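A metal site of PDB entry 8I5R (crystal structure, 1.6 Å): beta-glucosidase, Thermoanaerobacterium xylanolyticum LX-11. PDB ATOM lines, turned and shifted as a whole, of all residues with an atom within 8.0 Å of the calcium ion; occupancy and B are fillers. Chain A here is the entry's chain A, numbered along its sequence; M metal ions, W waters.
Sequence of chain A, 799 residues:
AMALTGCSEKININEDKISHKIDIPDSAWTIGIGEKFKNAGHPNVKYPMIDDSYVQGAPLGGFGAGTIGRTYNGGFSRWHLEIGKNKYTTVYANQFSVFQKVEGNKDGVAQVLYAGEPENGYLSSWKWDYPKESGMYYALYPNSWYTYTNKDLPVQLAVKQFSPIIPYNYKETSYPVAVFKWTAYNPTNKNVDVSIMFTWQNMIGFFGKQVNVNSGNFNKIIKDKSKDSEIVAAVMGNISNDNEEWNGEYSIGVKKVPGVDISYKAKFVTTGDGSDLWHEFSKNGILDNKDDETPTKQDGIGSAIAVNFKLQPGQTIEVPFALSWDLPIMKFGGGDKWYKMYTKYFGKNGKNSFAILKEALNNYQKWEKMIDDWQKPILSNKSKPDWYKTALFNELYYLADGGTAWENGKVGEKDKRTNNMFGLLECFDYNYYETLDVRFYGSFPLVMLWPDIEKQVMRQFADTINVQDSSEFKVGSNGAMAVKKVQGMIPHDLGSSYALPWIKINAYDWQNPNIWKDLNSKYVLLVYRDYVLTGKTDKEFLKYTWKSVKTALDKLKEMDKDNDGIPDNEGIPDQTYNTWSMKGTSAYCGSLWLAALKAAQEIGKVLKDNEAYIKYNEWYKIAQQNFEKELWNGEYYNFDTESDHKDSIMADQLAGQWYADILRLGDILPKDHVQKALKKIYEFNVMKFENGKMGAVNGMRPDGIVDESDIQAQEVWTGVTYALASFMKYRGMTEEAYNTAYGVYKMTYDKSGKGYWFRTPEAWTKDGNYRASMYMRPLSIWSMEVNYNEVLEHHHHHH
Five residues have an atom within 4 Å of the calcium ion: Asp 560, Asp 562, Asp 564, Ile 566 and Asp 568. The nearest printed residue that does not touch the calcium ion is Pro 567 (4.2 Å).
The calcium ion is bound by the side-chain carboxylate of Asp 568 (2.2 Å), the backbone carbonyl oxygen of Ile 566 (2.3 Å), the side-chain carboxylate of Asp 564 (2.3 Å), the side-chain carboxylate of Asp 560 (2.3 Å), water W1 (2.4 Å) and the side-chain carboxylate of Asp 562 (2.5 Å).
The backbone NH (N) of Gly 565 is in hydrogen-bond range of the side-chain carboxylate (OD2) of Asp 560, 2.8 Å away. The side-chain carboxylate (OD1) of Asp 568 sits close to the backbone NH (N) of Lys 561 (2.9 Å). The side-chain carboxylate (OD1) of Asp 560 sits close to the backbone NH (N) of Asn 563 (3.1 Å). The side-chain carboxylate of Asp 564 lies within hydrogen-bond range of the side-chain hydroxyl of Thr 585, 2.9 Å away. O of Asp 564 sits at hydrogen-bond distance from ND2 of Asn 626 (2.8 Å). The backbone NH (N) of Asp 568 lies within hydrogen-bond range of the backbone carbonyl oxygen (O) of Met 559. OD2 of Asp 564 sits close to OE2 of Glu 630.
Water W1 lies within hydrogen-bond range of the side-chain hydroxyl of Thr 585 (2.6 Å), the backbone carbonyl oxygen of Pro 567 (3.1 Å) and the side-chain carboxylate of Asp 568 (3.4 Å).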
ATOM      1  N   LYS A 557     -13.630  -1.390  32.536  1.00  0.00           N
ATOM      2  CA  LYS A 557     -13.399  -0.658  31.256  1.00  0.00           C
ATOM      3  C   LYS A 557     -12.487  -1.479  30.321  1.00  0.00           C
ATOM      4  O   LYS A 557     -12.675  -1.474  29.104  1.00  0.00           O
ATOM      5  CB  LYS A 557     -12.793   0.712  31.512  1.00  0.00           C
ATOM      6  CG  LYS A 557     -12.596   1.627  30.288  1.00  0.00           C
ATOM      7  CD  LYS A 557     -13.907   1.929  29.594  1.00  0.00           C
ATOM      8  CE  LYS A 557     -13.867   3.177  28.737  1.00  0.00           C
ATOM      9  NZ  LYS A 557     -12.862   3.081  27.657  1.00  0.00           N
ATOM     10  N   MET A 559     -12.625  -4.522  29.754  1.00  0.00           N
ATOM     11  CA  MET A 559     -13.394  -5.559  29.090  1.00  0.00           C
ATOM     12  C   MET A 559     -14.220  -5.045  27.911  1.00  0.00           C
ATOM     13  O   MET A 559     -14.980  -5.792  27.304  1.00  0.00           O
ATOM     14  CB  MET A 559     -14.292  -6.258  30.102  1.00  0.00           C
ATOM     15  CG  MET A 559     -13.508  -6.816  31.277  1.00  0.00           C
ATOM     16  SD  MET A 559     -14.631  -7.516  32.500  1.00  0.00           S
ATOM     17  CE  MET A 559     -13.494  -8.319  33.623  1.00  0.00           C
ATOM     18  N   ASP A 560     -14.071  -3.756  27.581  1.00  0.00           N
ATOM     19  CA  ASP A 560     -14.643  -3.204  26.353  1.00  0.00           C
ATOM     20  C   ASP A 560     -13.767  -3.589  25.145  1.00  0.00           C
ATOM     21  O   ASP A 560     -12.773  -2.941  24.895  1.00  0.00           O
ATOM     22  CB  ASP A 560     -14.774  -1.686  26.465  1.00  0.00           C
ATOM     23  CG  ASP A 560     -15.258  -1.046  25.186  1.00  0.00           C
ATOM     24  OD1 ASP A 560     -15.881  -1.723  24.347  1.00  0.00           O
ATOM     25  OD2 ASP A 560     -15.035   0.167  25.036  1.00  0.00           O
ATOM     26  N   LYS A 561     -14.181  -4.607  24.398  1.00  0.00           N
ATOM     27  CA  LYS A 561     -13.414  -5.163  23.258  1.00  0.00           C
ATOM     28  C   LYS A 561     -13.509  -4.330  21.985  1.00  0.00           C
ATOM     29  O   LYS A 561     -12.512  -4.177  21.284  1.00  0.00           O
ATOM     30  CB  LYS A 561     -13.889  -6.575  22.920  1.00  0.00           C
ATOM     31  CG  LYS A 561     -13.745  -7.601  24.035  1.00  0.00           C
ATOM     32  CD  LYS A 561     -12.298  -8.026  24.249  1.00  0.00           C
ATOM     33  CE  LYS A 561     -11.583  -7.223  25.343  1.00  0.00           C
ATOM     34  NZ  LYS A 561     -10.239  -7.815  25.599  1.00  0.00           N
ATOM     35  N   ASP A 562     -14.697  -3.831  21.676  1.00  0.00           N
ATOM     36  CA  ASP A 562     -14.969  -3.122  20.415  1.00  0.00           C
ATOM     37  C   ASP A 562     -14.919  -1.586  20.521  1.00  0.00           C
ATOM     38  O   ASP A 562     -15.327  -0.880  19.593  1.00  0.00           O
ATOM     39  CB  ASP A 562     -16.290  -3.602  19.821  1.00  0.00           C
ATOM     40  CG  ASP A 562     -17.508  -3.171  20.637  1.00  0.00           C
ATOM     41  OD1 ASP A 562     -17.337  -2.767  21.819  1.00  0.00           O
ATOM     42  OD2 ASP A 562     -18.628  -3.221  20.102  1.00  0.00           O
ATOM     43  N   ASN A 563     -14.415  -1.081  21.642  1.00  0.00           N
ATOM     44  CA  ASN A 563     -14.278   0.345  21.888  1.00  0.00           C
ATOM     45  C   ASN A 563     -15.529   1.258  21.792  1.00  0.00           C
ATOM     46  O   ASN A 563     -15.407   2.457  21.485  1.00  0.00           O
ATOM     47  CB  ASN A 563     -13.113   0.932  21.082  1.00  0.00           C
ATOM     48  CG  ASN A 563     -12.196   1.758  21.953  1.00  0.00           C
ATOM     49  OD1 ASN A 563     -11.402   1.203  22.737  1.00  0.00           O
ATOM     50  ND2 ASN A 563     -12.333   3.081  21.891  1.00  0.00           N
ATOM     51  N   ASP A 564     -16.711   0.710  22.095  1.00  0.00           N
ATOM     52  CA  ASP A 564     -17.947   1.528  22.196  1.00  0.00           C
ATOM     53  C   ASP A 564     -18.154   2.129  23.602  1.00  0.00           C
ATOM     54  O   ASP A 564     -19.181   2.760  23.842  1.00  0.00           O
ATOM     55  CB  ASP A 564     -19.196   0.736  21.772  1.00  0.00           C
ATOM     56  CG  ASP A 564     -19.622  -0.346  22.816  1.00  0.00           C
ATOM     57  OD1 ASP A 564     -18.848  -0.636  23.734  1.00  0.00           O
ATOM     58  OD2 ASP A 564     -20.702  -0.938  22.665  1.00  0.00           O
ATOM     59  N   GLY A 565     -17.196   1.925  24.496  1.00  0.00           N
ATOM     60  CA  GLY A 565     -17.202   2.534  25.819  1.00  0.00           C
ATOM     61  C   GLY A 565     -17.880   1.688  26.897  1.00  0.00           C
ATOM     62  O   GLY A 565     -18.011   2.131  28.039  1.00  0.00           O
ATOM     63  N   ILE A 566     -18.271   0.479  26.534  1.00  0.00           N
ATOM     64  CA  ILE A 566     -19.145  -0.375  27.378  1.00  0.00           C
ATOM     65  C   ILE A 566     -18.462  -1.734  27.453  1.00  0.00           C
ATOM     66  O   ILE A 566     -18.083  -2.276  26.415  1.00  0.00           O
ATOM     67  CB  ILE A 566     -20.540  -0.539  26.741  1.00  0.00           C
ATOM     68  CG1 ILE A 566     -21.214   0.826  26.522  1.00  0.00           C
ATOM     69  CG2 ILE A 566     -21.459  -1.427  27.612  1.00  0.00           C
ATOM     70  CD1 ILE A 566     -22.438   0.788  25.625  1.00  0.00           C
ATOM     71  N   PRO A 567     -18.321  -2.320  28.652  1.00  0.00           N
ATOM     72  CA  PRO A 567     -17.840  -3.714  28.687  1.00  0.00           C
ATOM     73  C   PRO A 567     -18.660  -4.659  27.831  1.00  0.00           C
ATOM     74  O   PRO A 567     -19.879  -4.508  27.724  1.00  0.00           O
ATOM     75  CB  PRO A 567     -17.928  -4.098  30.175  1.00  0.00           C
ATOM     76  CG  PRO A 567     -18.783  -3.055  30.804  1.00  0.00           C
ATOM     77  CD  PRO A 567     -18.683  -1.811  29.978  1.00  0.00           C
ATOM     78  N   ASP A 568     -17.986  -5.602  27.160  1.00  0.00           N
ATOM     79  CA  ASP A 568     -18.672  -6.550  26.303  1.00  0.00           C
ATOM     80  C   ASP A 568     -19.022  -7.809  27.035  1.00  0.00           C
ATOM     81  O   ASP A 568     -18.152  -8.448  27.627  1.00  0.00           O
ATOM     82  CB  ASP A 568     -17.779  -6.944  25.099  1.00  0.00           C
ATOM     83  CG  ASP A 568     -17.674  -5.837  24.074  1.00  0.00           C
ATOM     84  OD1 ASP A 568     -17.065  -4.777  24.400  1.00  0.00           O
ATOM     85  OD2 ASP A 568     -18.220  -6.014  22.958  1.00  0.00           O
ATOM     86  N   ASN A 569     -20.286  -8.211  26.975  1.00  0.00           N
ATOM     87  CA  ASN A 569     -20.644  -9.568  27.391  1.00  0.00           C
ATOM     88  C   ASN A 569     -20.136 -10.525  26.323  1.00  0.00           C
ATOM     89  O   ASN A 569     -20.124 -10.209  25.107  1.00  0.00           O
ATOM     90  CB  ASN A 569     -22.147  -9.702  27.605  1.00  0.00           C
ATOM     91  CG  ASN A 569     -22.639  -8.962  28.851  1.00  0.00           C
ATOM     92  OD1 ASN A 569     -23.159  -7.853  28.759  1.00  0.00           O
ATOM     93  ND2 ASN A 569     -22.467  -9.572  30.003  1.00  0.00           N
ATOM     94  N   GLY A 584     -22.204  -9.116  23.577  1.00  0.00           N
ATOM     95  CA  GLY A 584     -22.105  -7.737  23.092  1.00  0.00           C
ATOM     96  C   GLY A 584     -22.429  -6.741  24.188  1.00  0.00           C
ATOM     97  O   GLY A 584     -21.968  -6.871  25.313  1.00  0.00           O
ATOM     98  N   THR A 585     -23.174  -5.712  23.828  1.00  0.00           N
ATOM     99  CA  THR A 585     -23.674  -4.755  24.801  1.00  0.00           C
ATOM    100  C   THR A 585     -25.039  -5.277  25.236  1.00  0.00           C
ATOM    101  O   THR A 585     -25.904  -5.542  24.418  1.00  0.00           O
ATOM    102  CB  THR A 585     -23.788  -3.352  24.194  1.00  0.00           C
ATOM    103  OG1 THR A 585     -22.480  -2.817  23.969  1.00  0.00           O
ATOM    104  CG2 THR A 585     -24.482  -2.435  25.130  1.00  0.00           C
ATOM    105  N   TRP A 593     -23.590  -0.346  34.214  1.00  0.00           N
ATOM    106  CA  TRP A 593     -22.364   0.401  33.903  1.00  0.00           C
ATOM    107  C   TRP A 593     -22.579   1.928  33.830  1.00  0.00           C
ATOM    108  O   TRP A 593     -21.866   2.681  34.462  1.00  0.00           O
ATOM    109  CB  TRP A 593     -21.816  -0.156  32.598  1.00  0.00           C
ATOM    110  CG  TRP A 593     -20.576   0.548  31.995  1.00  0.00           C
ATOM    111  CD1 TRP A 593     -20.516   1.140  30.770  1.00  0.00           C
ATOM    112  CD2 TRP A 593     -19.269   0.671  32.571  1.00  0.00           C
ATOM    113  NE1 TRP A 593     -19.258   1.619  30.537  1.00  0.00           N
ATOM    114  CE2 TRP A 593     -18.470   1.360  31.635  1.00  0.00           C
ATOM    115  CE3 TRP A 593     -18.702   0.286  33.781  1.00  0.00           C
ATOM    116  CZ2 TRP A 593     -17.111   1.660  31.876  1.00  0.00           C
ATOM    117  CZ3 TRP A 593     -17.365   0.568  34.035  1.00  0.00           C
ATOM    118  CH2 TRP A 593     -16.573   1.253  33.066  1.00  0.00           C
ATOM    119  N   ASN A 626     -23.712   5.508  22.922  1.00  0.00           N
ATOM    120  CA  ASN A 626     -23.666   4.201  22.278  1.00  0.00           C
ATOM    121  C   ASN A 626     -24.714   3.221  22.771  1.00  0.00           C
ATOM    122  O   ASN A 626     -25.275   2.481  21.976  1.00  0.00           O
ATOM    123  CB  ASN A 626     -22.273   3.613  22.362  1.00  0.00           C
ATOM    124  CG  ASN A 626     -21.315   4.295  21.402  1.00  0.00           C
ATOM    125  OD1 ASN A 626     -21.751   4.754  20.345  1.00  0.00           O
ATOM    126  ND2 ASN A 626     -20.060   4.384  21.758  1.00  0.00           N
ATOM    127  N   GLU A 630     -27.299   1.520  20.173  1.00  0.00           N
ATOM    128  CA  GLU A 630     -27.230   0.093  19.976  1.00  0.00           C
ATOM    129  C   GLU A 630     -28.494  -0.667  20.393  1.00  0.00           C
ATOM    130  O   GLU A 630     -28.793  -1.701  19.831  1.00  0.00           O
ATOM    131  CB  GLU A 630     -26.042  -0.505  20.722  1.00  0.00           C
ATOM    132  CG  GLU A 630     -24.690  -0.108  20.153  1.00  0.00           C
ATOM    133  CD  GLU A 630     -23.560  -0.369  21.123  1.00  0.00           C
ATOM    134  OE1 GLU A 630     -23.783  -1.143  22.087  1.00  0.00           O
ATOM    135  OE2 GLU A 630     -22.467   0.194  20.961  1.00  0.00           O
ATOM    136  N   THR A 641     -26.911  -6.950  21.971  1.00  0.00           N
ATOM    137  CA  THR A 641     -26.591  -6.665  20.554  1.00  0.00           C
ATOM    138  C   THR A 641     -26.255  -7.895  19.728  1.00  0.00           C
ATOM    139  O   THR A 641     -26.314  -7.821  18.491  1.00  0.00           O
ATOM    140  CB  THR A 641     -25.432  -5.660  20.422  1.00  0.00           C
ATOM    141  OG1 THR A 641     -24.282  -6.115  21.144  1.00  0.00           O
ATOM    142  CG2 THR A 641     -25.826  -4.307  20.933  1.00  0.00           C
ATOM    143  N   GLU A 642     -25.893  -9.015  20.361  1.00  0.00           N
ATOM    144  CA  GLU A 642     -25.290 -10.154  19.616  1.00  0.00           C
ATOM    145  C   GLU A 642     -25.881 -11.559  19.827  1.00  0.00           C
ATOM    146  O   GLU A 642     -25.564 -12.457  19.071  1.00  0.00           O
ATOM    147  CB  GLU A 642     -23.772 -10.177  19.849  1.00  0.00           C
ATOM    148  CG  GLU A 642     -23.044  -8.971  19.251  1.00  0.00           C
ATOM    149  CD  GLU A 642     -21.549  -8.993  19.485  1.00  0.00           C
ATOM    150  OE1 GLU A 642     -20.945 -10.086  19.536  1.00  0.00           O
ATOM    151  OE2 GLU A 642     -20.963  -7.893  19.626  1.00  0.00           O
HETATM  152 CA    CA M   1     -17.975  -2.739  24.194  1.00  0.00          CA
HETATM  153  O   HOH W   1     -20.133  -3.736  24.696  1.00  0.00           O
